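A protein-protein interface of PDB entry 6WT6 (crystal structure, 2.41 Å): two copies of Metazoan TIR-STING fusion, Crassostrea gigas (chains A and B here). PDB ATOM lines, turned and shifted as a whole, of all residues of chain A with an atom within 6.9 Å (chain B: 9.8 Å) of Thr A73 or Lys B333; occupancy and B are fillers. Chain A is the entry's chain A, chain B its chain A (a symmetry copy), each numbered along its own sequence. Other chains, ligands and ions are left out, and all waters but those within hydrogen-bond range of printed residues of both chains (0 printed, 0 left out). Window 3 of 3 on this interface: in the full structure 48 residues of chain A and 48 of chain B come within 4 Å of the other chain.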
ATOM      1  N   PHE A  67      -5.146  -7.086  10.666  1.00  0.00           N
ATOM      2  CA  PHE A  67      -6.108  -5.989  10.726  1.00  0.00           C
ATOM      3  C   PHE A  67      -5.668  -4.983  11.784  1.00  0.00           C
ATOM      4  O   PHE A  67      -5.512  -5.336  12.960  1.00  0.00           O
ATOM      5  CB  PHE A  67      -7.521  -6.498  11.021  1.00  0.00           C
ATOM      6  CG  PHE A  67      -8.122  -7.311   9.905  1.00  0.00           C
ATOM      7  CD1 PHE A  67      -7.517  -7.357   8.659  1.00  0.00           C
ATOM      8  CD2 PHE A  67      -9.294  -8.026  10.101  1.00  0.00           C
ATOM      9  CE1 PHE A  67      -8.061  -8.106   7.632  1.00  0.00           C
ATOM     10  CE2 PHE A  67      -9.846  -8.776   9.074  1.00  0.00           C
ATOM     11  CZ  PHE A  67      -9.226  -8.816   7.839  1.00  0.00           C
ATOM     12  N   LEU A  68      -5.465  -3.732  11.362  1.00  0.00           N
ATOM     13  CA  LEU A  68      -5.080  -2.673  12.280  1.00  0.00           C
ATOM     14  C   LEU A  68      -6.169  -2.482  13.335  1.00  0.00           C
ATOM     15  O   LEU A  68      -7.331  -2.826  13.104  1.00  0.00           O
ATOM     16  CB  LEU A  68      -4.830  -1.375  11.512  1.00  0.00           C
ATOM     17  CG  LEU A  68      -3.801  -1.461  10.376  1.00  0.00           C
ATOM     18  CD1 LEU A  68      -4.488  -1.664   9.029  1.00  0.00           C
ATOM     19  CD2 LEU A  68      -2.891  -0.241  10.346  1.00  0.00           C
ATOM     20  N   GLY A  70      -8.060  -0.156  14.483  1.00  0.00           N
ATOM     21  CA  GLY A  70      -9.256   0.600  14.176  1.00  0.00           C
ATOM     22  C   GLY A  70      -9.941   0.271  12.868  1.00  0.00           C
ATOM     23  O   GLY A  70     -10.882   0.980  12.490  1.00  0.00           O
ATOM     24  N   GLU A  71      -9.519  -0.784  12.168  1.00  0.00           N
ATOM     25  CA  GLU A  71     -10.019  -1.084  10.831  1.00  0.00           C
ATOM     26  C   GLU A  71     -10.560  -2.507  10.723  1.00  0.00           C
ATOM     27  O   GLU A  71     -10.518  -3.111   9.648  1.00  0.00           O
ATOM     28  CB  GLU A  71      -8.930  -0.850   9.787  1.00  0.00           C
ATOM     29  CG  GLU A  71      -8.520   0.604   9.657  1.00  0.00           C
ATOM     30  CD  GLU A  71      -9.667   1.488   9.205  1.00  0.00           C
ATOM     31  OE1 GLU A  71     -10.472   1.036   8.360  1.00  0.00           O
ATOM     32  OE2 GLU A  71      -9.771   2.632   9.699  1.00  0.00           O
ATOM     33  N   CYS A  72     -11.078  -3.057  11.817  1.00  0.00           N
ATOM     34  CA  CYS A  72     -11.680  -4.391  11.783  1.00  0.00           C
ATOM     35  C   CYS A  72     -13.166  -4.320  11.441  1.00  0.00           C
ATOM     36  O   CYS A  72     -14.023  -4.851  12.147  1.00  0.00           O
ATOM     37  CB  CYS A  72     -11.453  -5.102  13.111  1.00  0.00           C
ATOM     38  SG  CYS A  72     -11.703  -6.898  13.018  1.00  0.00           S
ATOM     39  N   THR A  73     -13.478  -3.655  10.336  1.00  0.00           N
ATOM     40  CA  THR A  73     -14.850  -3.529   9.874  1.00  0.00           C
ATOM     41  C   THR A  73     -15.176  -4.637   8.870  1.00  0.00           C
ATOM     42  O   THR A  73     -14.302  -5.373   8.407  1.00  0.00           O
ATOM     43  CB  THR A  73     -15.085  -2.140   9.270  1.00  0.00           C
ATOM     44  OG1 THR A  73     -14.258  -1.965   8.115  1.00  0.00           O
ATOM     45  CG2 THR A  73     -14.738  -1.059  10.284  1.00  0.00           C
ATOM     46  N   SER A  74     -16.467  -4.747   8.536  1.00  0.00           N
ATOM     47  CA  SER A  74     -16.921  -5.836   7.675  1.00  0.00           C
ATOM     48  C   SER A  74     -16.357  -5.728   6.265  1.00  0.00           C
ATOM     49  O   SER A  74     -16.148  -6.756   5.607  1.00  0.00           O
ATOM     50  CB  SER A  74     -18.449  -5.866   7.620  1.00  0.00           C
ATOM     51  OG  SER A  74     -18.953  -4.671   7.044  1.00  0.00           O
ATOM     52  N   ASP A  75     -16.110  -4.505   5.787  1.00  0.00           N
ATOM     53  CA  ASP A  75     -15.611  -4.325   4.426  1.00  0.00           C
ATOM     54  C   ASP A  75     -14.138  -4.695   4.305  1.00  0.00           C
ATOM     55  O   ASP A  75     -13.699  -5.200   3.266  1.00  0.00           O
ATOM     56  CB  ASP A  75     -15.825  -2.883   3.981  1.00  0.00           C
ATOM     57  CG  ASP A  75     -15.142  -1.878   4.894  1.00  0.00           C
ATOM     58  OD1 ASP A  75     -15.358  -1.994   6.116  1.00  0.00           O
ATOM     59  OD2 ASP A  75     -14.417  -0.989   4.394  1.00  0.00           O
ATOM     60  N   VAL A  76     -13.350  -4.402   5.340  1.00  0.00           N
ATOM     61  CA  VAL A  76     -11.967  -4.869   5.370  1.00  0.00           C
ATOM     62  C   VAL A  76     -11.932  -6.392   5.403  1.00  0.00           C
ATOM     63  O   VAL A  76     -11.068  -7.027   4.782  1.00  0.00           O
ATOM     64  CB  VAL A  76     -11.219  -4.254   6.570  1.00  0.00           C
ATOM     65  CG1 VAL A  76      -9.835  -4.864   6.723  1.00  0.00           C
ATOM     66  CG2 VAL A  76     -11.124  -2.745   6.413  1.00  0.00           C
ATOM     67  N   VAL A  77     -12.888  -7.002   6.108  1.00  0.00           N
ATOM     68  CA  VAL A  77     -12.996  -8.457   6.116  1.00  0.00           C
ATOM     69  C   VAL A  77     -13.290  -8.973   4.713  1.00  0.00           C
ATOM     70  O   VAL A  77     -12.621  -9.885   4.213  1.00  0.00           O
ATOM     71  CB  VAL A  77     -14.068  -8.909   7.124  1.00  0.00           C
ATOM     72  CG1 VAL A  77     -14.390 -10.386   6.945  1.00  0.00           C
ATOM     73  CG2 VAL A  77     -13.602  -8.634   8.547  1.00  0.00           C
ATOM     74  N   VAL A  78     -14.285  -8.383   4.051  1.00  0.00           N
ATOM     75  CA  VAL A  78     -14.650  -8.836   2.715  1.00  0.00           C
ATOM     76  C   VAL A  78     -13.536  -8.534   1.719  1.00  0.00           C
ATOM     77  O   VAL A  78     -13.298  -9.315   0.788  1.00  0.00           O
ATOM     78  CB  VAL A  78     -15.998  -8.216   2.301  1.00  0.00           C
ATOM     79  CG1 VAL A  78     -16.284  -8.465   0.832  1.00  0.00           C
ATOM     80  CG2 VAL A  78     -17.105  -8.807   3.157  1.00  0.00           C
ATOM     81  N   GLU A 104     -20.230 -12.549  10.328  1.00  0.00           N
ATOM     82  CA  GLU A 104     -18.992 -12.629   9.558  1.00  0.00           C
ATOM     83  C   GLU A 104     -18.842 -13.980   8.874  1.00  0.00           C
ATOM     84  O   GLU A 104     -18.275 -14.063   7.779  1.00  0.00           O
ATOM     85  CB  GLU A 104     -17.787 -12.355  10.455  1.00  0.00           C
ATOM     86  CG  GLU A 104     -16.518 -12.080   9.675  1.00  0.00           C
ATOM     87  CD  GLU A 104     -15.272 -12.120  10.534  1.00  0.00           C
ATOM     88  OE1 GLU A 104     -15.131 -11.268  11.439  1.00  0.00           O
ATOM     89  OE2 GLU A 104     -14.423 -13.007  10.297  1.00  0.00           O
ATOM     90  N   PHE B 219     -20.144   4.938  -4.236  1.00  0.00           N
ATOM     91  CA  PHE B 219     -20.308   5.141  -2.804  1.00  0.00           C
ATOM     92  C   PHE B 219     -21.304   4.141  -2.238  1.00  0.00           C
ATOM     93  O   PHE B 219     -22.402   3.964  -2.778  1.00  0.00           O
ATOM     94  CB  PHE B 219     -20.734   6.580  -2.511  1.00  0.00           C
ATOM     95  CG  PHE B 219     -19.641   7.577  -2.767  1.00  0.00           C
ATOM     96  CD1 PHE B 219     -18.732   7.895  -1.771  1.00  0.00           C
ATOM     97  CD2 PHE B 219     -19.492   8.158  -4.014  1.00  0.00           C
ATOM     98  CE1 PHE B 219     -17.710   8.797  -2.010  1.00  0.00           C
ATOM     99  CE2 PHE B 219     -18.474   9.062  -4.257  1.00  0.00           C
ATOM    100  CZ  PHE B 219     -17.581   9.380  -3.255  1.00  0.00           C
ATOM    101  N   PHE B 220     -20.907   3.497  -1.141  1.00  0.00           N
ATOM    102  CA  PHE B 220     -21.630   2.375  -0.545  1.00  0.00           C
ATOM    103  C   PHE B 220     -21.783   2.675   0.942  1.00  0.00           C
ATOM    104  O   PHE B 220     -21.011   2.172   1.771  1.00  0.00           O
ATOM    105  CB  PHE B 220     -20.875   1.064  -0.795  1.00  0.00           C
ATOM    106  CG  PHE B 220     -21.685  -0.188  -0.565  1.00  0.00           C
ATOM    107  CD1 PHE B 220     -22.615  -0.275   0.465  1.00  0.00           C
ATOM    108  CD2 PHE B 220     -21.494  -1.296  -1.377  1.00  0.00           C
ATOM    109  CE1 PHE B 220     -23.343  -1.435   0.667  1.00  0.00           C
ATOM    110  CE2 PHE B 220     -22.215  -2.457  -1.178  1.00  0.00           C
ATOM    111  CZ  PHE B 220     -23.144  -2.529  -0.156  1.00  0.00           C
ATOM    112  N   PRO B 221     -22.760   3.501   1.314  1.00  0.00           N
ATOM    113  CA  PRO B 221     -23.025   3.730   2.740  1.00  0.00           C
ATOM    114  C   PRO B 221     -23.536   2.461   3.405  1.00  0.00           C
ATOM    115  O   PRO B 221     -24.345   1.725   2.836  1.00  0.00           O
ATOM    116  CB  PRO B 221     -24.093   4.827   2.730  1.00  0.00           C
ATOM    117  CG  PRO B 221     -24.775   4.665   1.404  1.00  0.00           C
ATOM    118  CD  PRO B 221     -23.690   4.248   0.450  1.00  0.00           C
ATOM    119  N   GLN B 222     -23.060   2.213   4.632  1.00  0.00           N
ATOM    120  CA  GLN B 222     -23.407   0.969   5.316  1.00  0.00           C
ATOM    121  C   GLN B 222     -24.906   0.849   5.558  1.00  0.00           C
ATOM    122  O   GLN B 222     -25.445  -0.262   5.567  1.00  0.00           O
ATOM    123  CB  GLN B 222     -22.653   0.864   6.642  1.00  0.00           C
ATOM    124  CG  GLN B 222     -22.938  -0.423   7.404  1.00  0.00           C
ATOM    125  CD  GLN B 222     -22.128  -0.542   8.676  1.00  0.00           C
ATOM    126  OE1 GLN B 222     -21.337   0.338   9.004  1.00  0.00           O
ATOM    127  NE2 GLN B 222     -22.322  -1.636   9.401  1.00  0.00           N
ATOM    128  N   SER B 223     -25.597   1.968   5.771  1.00  0.00           N
ATOM    129  CA  SER B 223     -27.037   1.890   5.968  1.00  0.00           C
ATOM    130  C   SER B 223     -27.783   1.586   4.679  1.00  0.00           C
ATOM    131  O   SER B 223     -28.987   1.310   4.735  1.00  0.00           O
ATOM    132  CB  SER B 223     -27.571   3.193   6.558  1.00  0.00           C
ATOM    133  OG  SER B 223     -27.660   4.188   5.554  1.00  0.00           O
ATOM    134  N   CYS B 224     -27.095   1.645   3.534  1.00  0.00           N
ATOM    135  CA  CYS B 224     -27.636   1.478   2.188  1.00  0.00           C
ATOM    136  C   CYS B 224     -28.577   2.607   1.786  1.00  0.00           C
ATOM    137  O   CYS B 224     -29.211   2.523   0.725  1.00  0.00           O
ATOM    138  CB  CYS B 224     -28.340   0.125   2.023  1.00  0.00           C
ATOM    139  SG  CYS B 224     -27.258  -1.270   2.415  1.00  0.00           S
ATOM    140  N   ARG B 225     -28.691   3.659   2.598  1.00  0.00           N
ATOM    141  CA  ARG B 225     -29.475   4.827   2.222  1.00  0.00           C
ATOM    142  C   ARG B 225     -28.713   5.637   1.187  1.00  0.00           C
ATOM    143  O   ARG B 225     -27.617   6.138   1.460  1.00  0.00           O
ATOM    144  CB  ARG B 225     -29.774   5.694   3.442  1.00  0.00           C
ATOM    145  CG  ARG B 225     -30.868   5.176   4.332  1.00  0.00           C
ATOM    146  CD  ARG B 225     -31.066   6.074   5.544  1.00  0.00           C
ATOM    147  NE  ARG B 225     -29.847   6.205   6.336  1.00  0.00           N
ATOM    148  CZ  ARG B 225     -29.702   7.058   7.346  1.00  0.00           C
ATOM    149  NH1 ARG B 225     -30.704   7.855   7.690  1.00  0.00           N
ATOM    150  NH2 ARG B 225     -28.553   7.115   8.010  1.00  0.00           N
ATOM    151  N   GLU B 233     -23.975  15.246   1.344  1.00  0.00           N
ATOM    152  CA  GLU B 233     -23.331  14.876   2.598  1.00  0.00           C
ATOM    153  C   GLU B 233     -22.519  16.012   3.197  1.00  0.00           C
ATOM    154  O   GLU B 233     -22.237  15.985   4.401  1.00  0.00           O
ATOM    155  CB  GLU B 233     -22.419  13.665   2.391  1.00  0.00           C
ATOM    156  CG  GLU B 233     -23.133  12.329   2.459  1.00  0.00           C
ATOM    157  CD  GLU B 233     -23.411  11.887   3.883  1.00  0.00           C
ATOM    158  OE1 GLU B 233     -22.743  12.392   4.809  1.00  0.00           O
ATOM    159  OE2 GLU B 233     -24.301  11.035   4.074  1.00  0.00           O
ATOM    160  N   TYR B 303     -26.996  -6.010   6.475  1.00  0.00           N
ATOM    161  CA  TYR B 303     -25.538  -5.965   6.420  1.00  0.00           C
ATOM    162  C   TYR B 303     -24.971  -7.194   5.718  1.00  0.00           C
ATOM    163  O   TYR B 303     -24.050  -7.077   4.903  1.00  0.00           O
ATOM    164  CB  TYR B 303     -24.965  -5.843   7.831  1.00  0.00           C
ATOM    165  CG  TYR B 303     -25.333  -4.558   8.537  1.00  0.00           C
ATOM    166  CD1 TYR B 303     -25.534  -3.386   7.823  1.00  0.00           C
ATOM    167  CD2 TYR B 303     -25.477  -4.518   9.917  1.00  0.00           C
ATOM    168  CE1 TYR B 303     -25.867  -2.211   8.459  1.00  0.00           C
ATOM    169  CE2 TYR B 303     -25.813  -3.340  10.565  1.00  0.00           C
ATOM    170  CZ  TYR B 303     -26.007  -2.191   9.828  1.00  0.00           C
ATOM    171  OH  TYR B 303     -26.339  -1.015  10.457  1.00  0.00           O
ATOM    172  N   MET B 307     -22.929  -7.145   2.102  1.00  0.00           N
ATOM    173  CA  MET B 307     -21.538  -7.578   1.968  1.00  0.00           C
ATOM    174  C   MET B 307     -21.391  -8.721   0.967  1.00  0.00           C
ATOM    175  O   MET B 307     -20.356  -8.824   0.300  1.00  0.00           O
ATOM    176  CB  MET B 307     -20.959  -7.998   3.324  1.00  0.00           C
ATOM    177  CG  MET B 307     -20.813  -6.852   4.322  1.00  0.00           C
ATOM    178  SD  MET B 307     -20.279  -5.312   3.540  1.00  0.00           S
ATOM    179  CE  MET B 307     -18.569  -5.655   3.225  1.00  0.00           C
ATOM    180  N   TYR B 310     -21.518  -6.831  -2.187  1.00  0.00           N
ATOM    181  CA  TYR B 310     -20.228  -6.168  -2.338  1.00  0.00           C
ATOM    182  C   TYR B 310     -19.161  -7.143  -2.818  1.00  0.00           C
ATOM    183  O   TYR B 310     -18.378  -6.829  -3.722  1.00  0.00           O
ATOM    184  CB  TYR B 310     -19.844  -5.533  -0.997  1.00  0.00           C
ATOM    185  CG  TYR B 310     -18.512  -4.825  -0.951  1.00  0.00           C
ATOM    186  CD1 TYR B 310     -18.263  -3.713  -1.741  1.00  0.00           C
ATOM    187  CD2 TYR B 310     -17.517  -5.247  -0.082  1.00  0.00           C
ATOM    188  CE1 TYR B 310     -17.049  -3.061  -1.684  1.00  0.00           C
ATOM    189  CE2 TYR B 310     -16.303  -4.601  -0.018  1.00  0.00           C
ATOM    190  CZ  TYR B 310     -16.074  -3.508  -0.820  1.00  0.00           C
ATOM    191  OH  TYR B 310     -14.863  -2.863  -0.759  1.00  0.00           O
ATOM    192  N   VAL B 330     -16.451   2.712  -2.577  1.00  0.00           N
ATOM    193  CA  VAL B 330     -16.137   3.399  -1.326  1.00  0.00           C
ATOM    194  C   VAL B 330     -17.192   2.990  -0.305  1.00  0.00           C
ATOM    195  O   VAL B 330     -18.287   3.565  -0.259  1.00  0.00           O
ATOM    196  CB  VAL B 330     -16.098   4.923  -1.502  1.00  0.00           C
ATOM    197  CG1 VAL B 330     -15.752   5.614  -0.174  1.00  0.00           C
ATOM    198  CG2 VAL B 330     -15.117   5.318  -2.604  1.00  0.00           C
ATOM    199  N   PHE B 331     -16.876   1.999   0.523  1.00  0.00           N
ATOM    200  CA  PHE B 331     -17.746   1.626   1.630  1.00  0.00           C
ATOM    201  C   PHE B 331     -17.399   2.470   2.852  1.00  0.00           C
ATOM    202  O   PHE B 331     -16.218   2.648   3.177  1.00  0.00           O
ATOM    203  CB  PHE B 331     -17.610   0.138   1.947  1.00  0.00           C
ATOM    204  CG  PHE B 331     -18.532  -0.338   3.038  1.00  0.00           C
ATOM    205  CD1 PHE B 331     -19.793  -0.820   2.736  1.00  0.00           C
ATOM    206  CD2 PHE B 331     -18.132  -0.302   4.368  1.00  0.00           C
ATOM    207  CE1 PHE B 331     -20.641  -1.258   3.738  1.00  0.00           C
ATOM    208  CE2 PHE B 331     -18.974  -0.738   5.373  1.00  0.00           C
ATOM    209  CZ  PHE B 331     -20.229  -1.216   5.059  1.00  0.00           C
ATOM    210  N   TYR B 332     -18.425   2.979   3.532  1.00  0.00           N
ATOM    211  CA  TYR B 332     -18.195   3.855   4.671  1.00  0.00           C
ATOM    212  C   TYR B 332     -19.398   3.810   5.596  1.00  0.00           C
ATOM    213  O   TYR B 332     -20.527   3.561   5.160  1.00  0.00           O
ATOM    214  CB  TYR B 332     -17.928   5.294   4.223  1.00  0.00           C
ATOM    215  CG  TYR B 332     -19.087   5.932   3.484  1.00  0.00           C
ATOM    216  CD1 TYR B 332     -19.267   5.730   2.116  1.00  0.00           C
ATOM    217  CD2 TYR B 332     -20.002   6.741   4.153  1.00  0.00           C
ATOM    218  CE1 TYR B 332     -20.327   6.310   1.438  1.00  0.00           C
ATOM    219  CE2 TYR B 332     -21.066   7.320   3.487  1.00  0.00           C
ATOM    220  CZ  TYR B 332     -21.223   7.107   2.130  1.00  0.00           C
ATOM    221  OH  TYR B 332     -22.280   7.689   1.467  1.00  0.00           O
ATOM    222  N   LYS B 333     -19.140   4.062   6.880  1.00  0.00           N
ATOM    223  CA  LYS B 333     -20.197   4.219   7.875  1.00  0.00           C
ATOM    224  C   LYS B 333     -20.771   5.624   7.755  1.00  0.00           C
ATOM    225  O   LYS B 333     -20.103   6.606   8.099  1.00  0.00           O
ATOM    226  CB  LYS B 333     -19.663   3.981   9.285  1.00  0.00           C
ATOM    227  CG  LYS B 333     -19.031   2.620   9.498  1.00  0.00           C
ATOM    228  CD  LYS B 333     -18.775   2.346  10.976  1.00  0.00           C
ATOM    229  CE  LYS B 333     -17.952   1.079  11.167  1.00  0.00           C
ATOM    230  NZ  LYS B 333     -17.928   0.630  12.585  1.00  0.00           N
ATOM    231  N   ASP B 334     -22.010   5.722   7.277  1.00  0.00           N
ATOM    232  CA  ASP B 334     -22.662   7.020   7.105  1.00  0.00           C
ATOM    233  C   ASP B 334     -23.292   7.440   8.435  1.00  0.00           C
ATOM    234  O   ASP B 334     -24.509   7.417   8.626  1.00  0.00           O
ATOM    235  CB  ASP B 334     -23.686   6.957   5.977  1.00  0.00           C
ATOM    236  CG  ASP B 334     -24.613   5.764   6.095  1.00  0.00           C
ATOM    237  OD1 ASP B 334     -24.175   4.714   6.598  1.00  0.00           O
ATOM    238  OD2 ASP B 334     -25.783   5.875   5.680  1.00  0.00           O
ATOM    239  N   VAL B 335     -22.423   7.837   9.365  1.00  0.00           N
ATOM    240  CA  VAL B 335     -22.836   8.193  10.719  1.00  0.00           C
ATOM    241  C   VAL B 335     -22.434   9.604  11.126  1.00  0.00           C
ATOM    242  O   VAL B 335     -22.812  10.041  12.223  1.00  0.00           O
ATOM    243  CB  VAL B 335     -22.294   7.184  11.760  1.00  0.00           C
ATOM    244  CG1 VAL B 335     -22.789   5.772  11.470  1.00  0.00           C
ATOM    245  CG2 VAL B 335     -20.765   7.232  11.811  1.00  0.00           C
ATOM    246  N   ASN B 336     -21.682  10.335  10.307  1.00  0.00           N
ATOM    247  CA  ASN B 336     -21.093  11.604  10.717  1.00  0.00           C
ATOM    248  C   ASN B 336     -21.766  12.783  10.023  1.00  0.00           C
ATOM    249  O   ASN B 336     -22.094  12.717   8.834  1.00  0.00           O
ATOM    250  CB  ASN B 336     -19.593  11.627  10.420  1.00  0.00           C
ATOM    251  CG  ASN B 336     -18.804  10.727  11.345  1.00  0.00           C
ATOM    252  OD1 ASN B 336     -18.973  10.773  12.566  1.00  0.00           O
ATOM    253  ND2 ASN B 336     -17.938   9.900  10.770  1.00  0.00           N
ATOM    254  N   ASN B 337     -21.946  13.871  10.776  1.00  0.00           N
ATOM    255  CA  ASN B 337     -22.569  15.087  10.271  1.00  0.00           C
ATOM    256  C   ASN B 337     -21.594  16.224  10.006  1.00  0.00           C
ATOM    257  O   ASN B 337     -21.963  17.171   9.305  1.00  0.00           O
ATOM    258  CB  ASN B 337     -23.633  15.598  11.254  1.00  0.00           C
ATOM    259  CG  ASN B 337     -24.788  14.643  11.408  1.00  0.00           C
ATOM    260  OD1 ASN B 337     -25.152  13.938  10.470  1.00  0.00           O
ATOM    261  ND2 ASN B 337     -25.377  14.618  12.596  1.00  0.00           N
ATOM    262  N   ALA B 341     -16.033  15.427   7.522  1.00  0.00           N
ATOM    263  CA  ALA B 341     -15.920  13.974   7.577  1.00  0.00           C
ATOM    264  C   ALA B 341     -15.912  13.363   6.180  1.00  0.00           C
ATOM    265  O   ALA B 341     -14.977  12.646   5.809  1.00  0.00           O
ATOM    266  CB  ALA B 341     -17.055  13.400   8.427  1.00  0.00           C
ATOM    267  N   MET B 342     -16.952  13.631   5.392  1.00  0.00           N
ATOM    268  CA  MET B 342     -17.040  13.030   4.064  1.00  0.00           C
ATOM    269  C   MET B 342     -15.975  13.599   3.129  1.00  0.00           C
ATOM    270  O   MET B 342     -15.348  12.829   2.389  1.00  0.00           O
ATOM    271  CB  MET B 342     -18.440  13.211   3.468  1.00  0.00           C
ATOM    272  CG  MET B 342     -18.629  12.535   2.122  1.00  0.00           C
ATOM    273  SD  MET B 342     -18.634  10.739   2.251  1.00  0.00           S
ATOM    274  CE  MET B 342     -19.967  10.520   3.421  1.00  0.00           C
ATOM    275  N   LEU B 345     -12.730  11.762   3.877  1.00  0.00           N
ATOM    276  CA  LEU B 345     -12.746  10.381   3.414  1.00  0.00           C
ATOM    277  C   LEU B 345     -12.466  10.301   1.917  1.00  0.00           C
ATOM    278  O   LEU B 345     -11.672   9.468   1.467  1.00  0.00           O
ATOM    279  CB  LEU B 345     -14.090   9.739   3.750  1.00  0.00           C
ATOM    280  CG  LEU B 345     -14.346   8.403   3.051  1.00  0.00           C
ATOM    281  CD1 LEU B 345     -13.347   7.359   3.527  1.00  0.00           C
ATOM    282  CD2 LEU B 345     -15.773   7.945   3.286  1.00  0.00           C
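Among the printed residues, merely in contact across the chains: Asp A75 with Phe B331 (3.4 Å), Asp A75 with Met B307 (3.5 Å), Val A78 with Met B307 (3.5 Å), Val A78 with Tyr B310 (3.6 Å), Ser A74 with Met B307 (3.6 Å) and Thr A73 with Lys B333 (3.96 Å).
Of chain A, only Thr A73 (3.96 Å) comes within 4 Å of Lys B333. No residue of chain B comes within 4 Å of Cys A72. Asp A75 touches just these residues of chain B: Met B307 (3.5 Å) and Phe B331 (3.4 Å). No residue of chain B comes within 4 Å of Val A76. Printed residues of chain A within 4 Å of Phe B331: Asp A75. Printed residues of chain A within 4 Å of Met B307: Ser A74 (3.6 Å), Asp A75 (3.5 Å) and Val A78 (3.5 Å). Of the printed residues of chain B, Val A78 touches Met B307 and Tyr B310. Of the printed residues of chain A, Tyr B310 touches Val A78. Gly A70 touches none of the printed residues of chain B. The nearest residue of chain A that does not touch Lys B333 is Asp A75 (6.5 Å). The nearest printed residue of chain A that does not touch Phe B331 is Ser A74 (4.2 Å).
Of the 22 printed residues of chain B, 4 touch a printed residue of chain A. Hydrophobic or aromatic side chains of chain B within 4 Å of the printed part of chain A: Met B307, Tyr B310 and Phe B331.
No position is printed for both chains. Of the 6 pairs that touch across the chains among the printed residues, none has its exchanged pair printed and touching as well.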
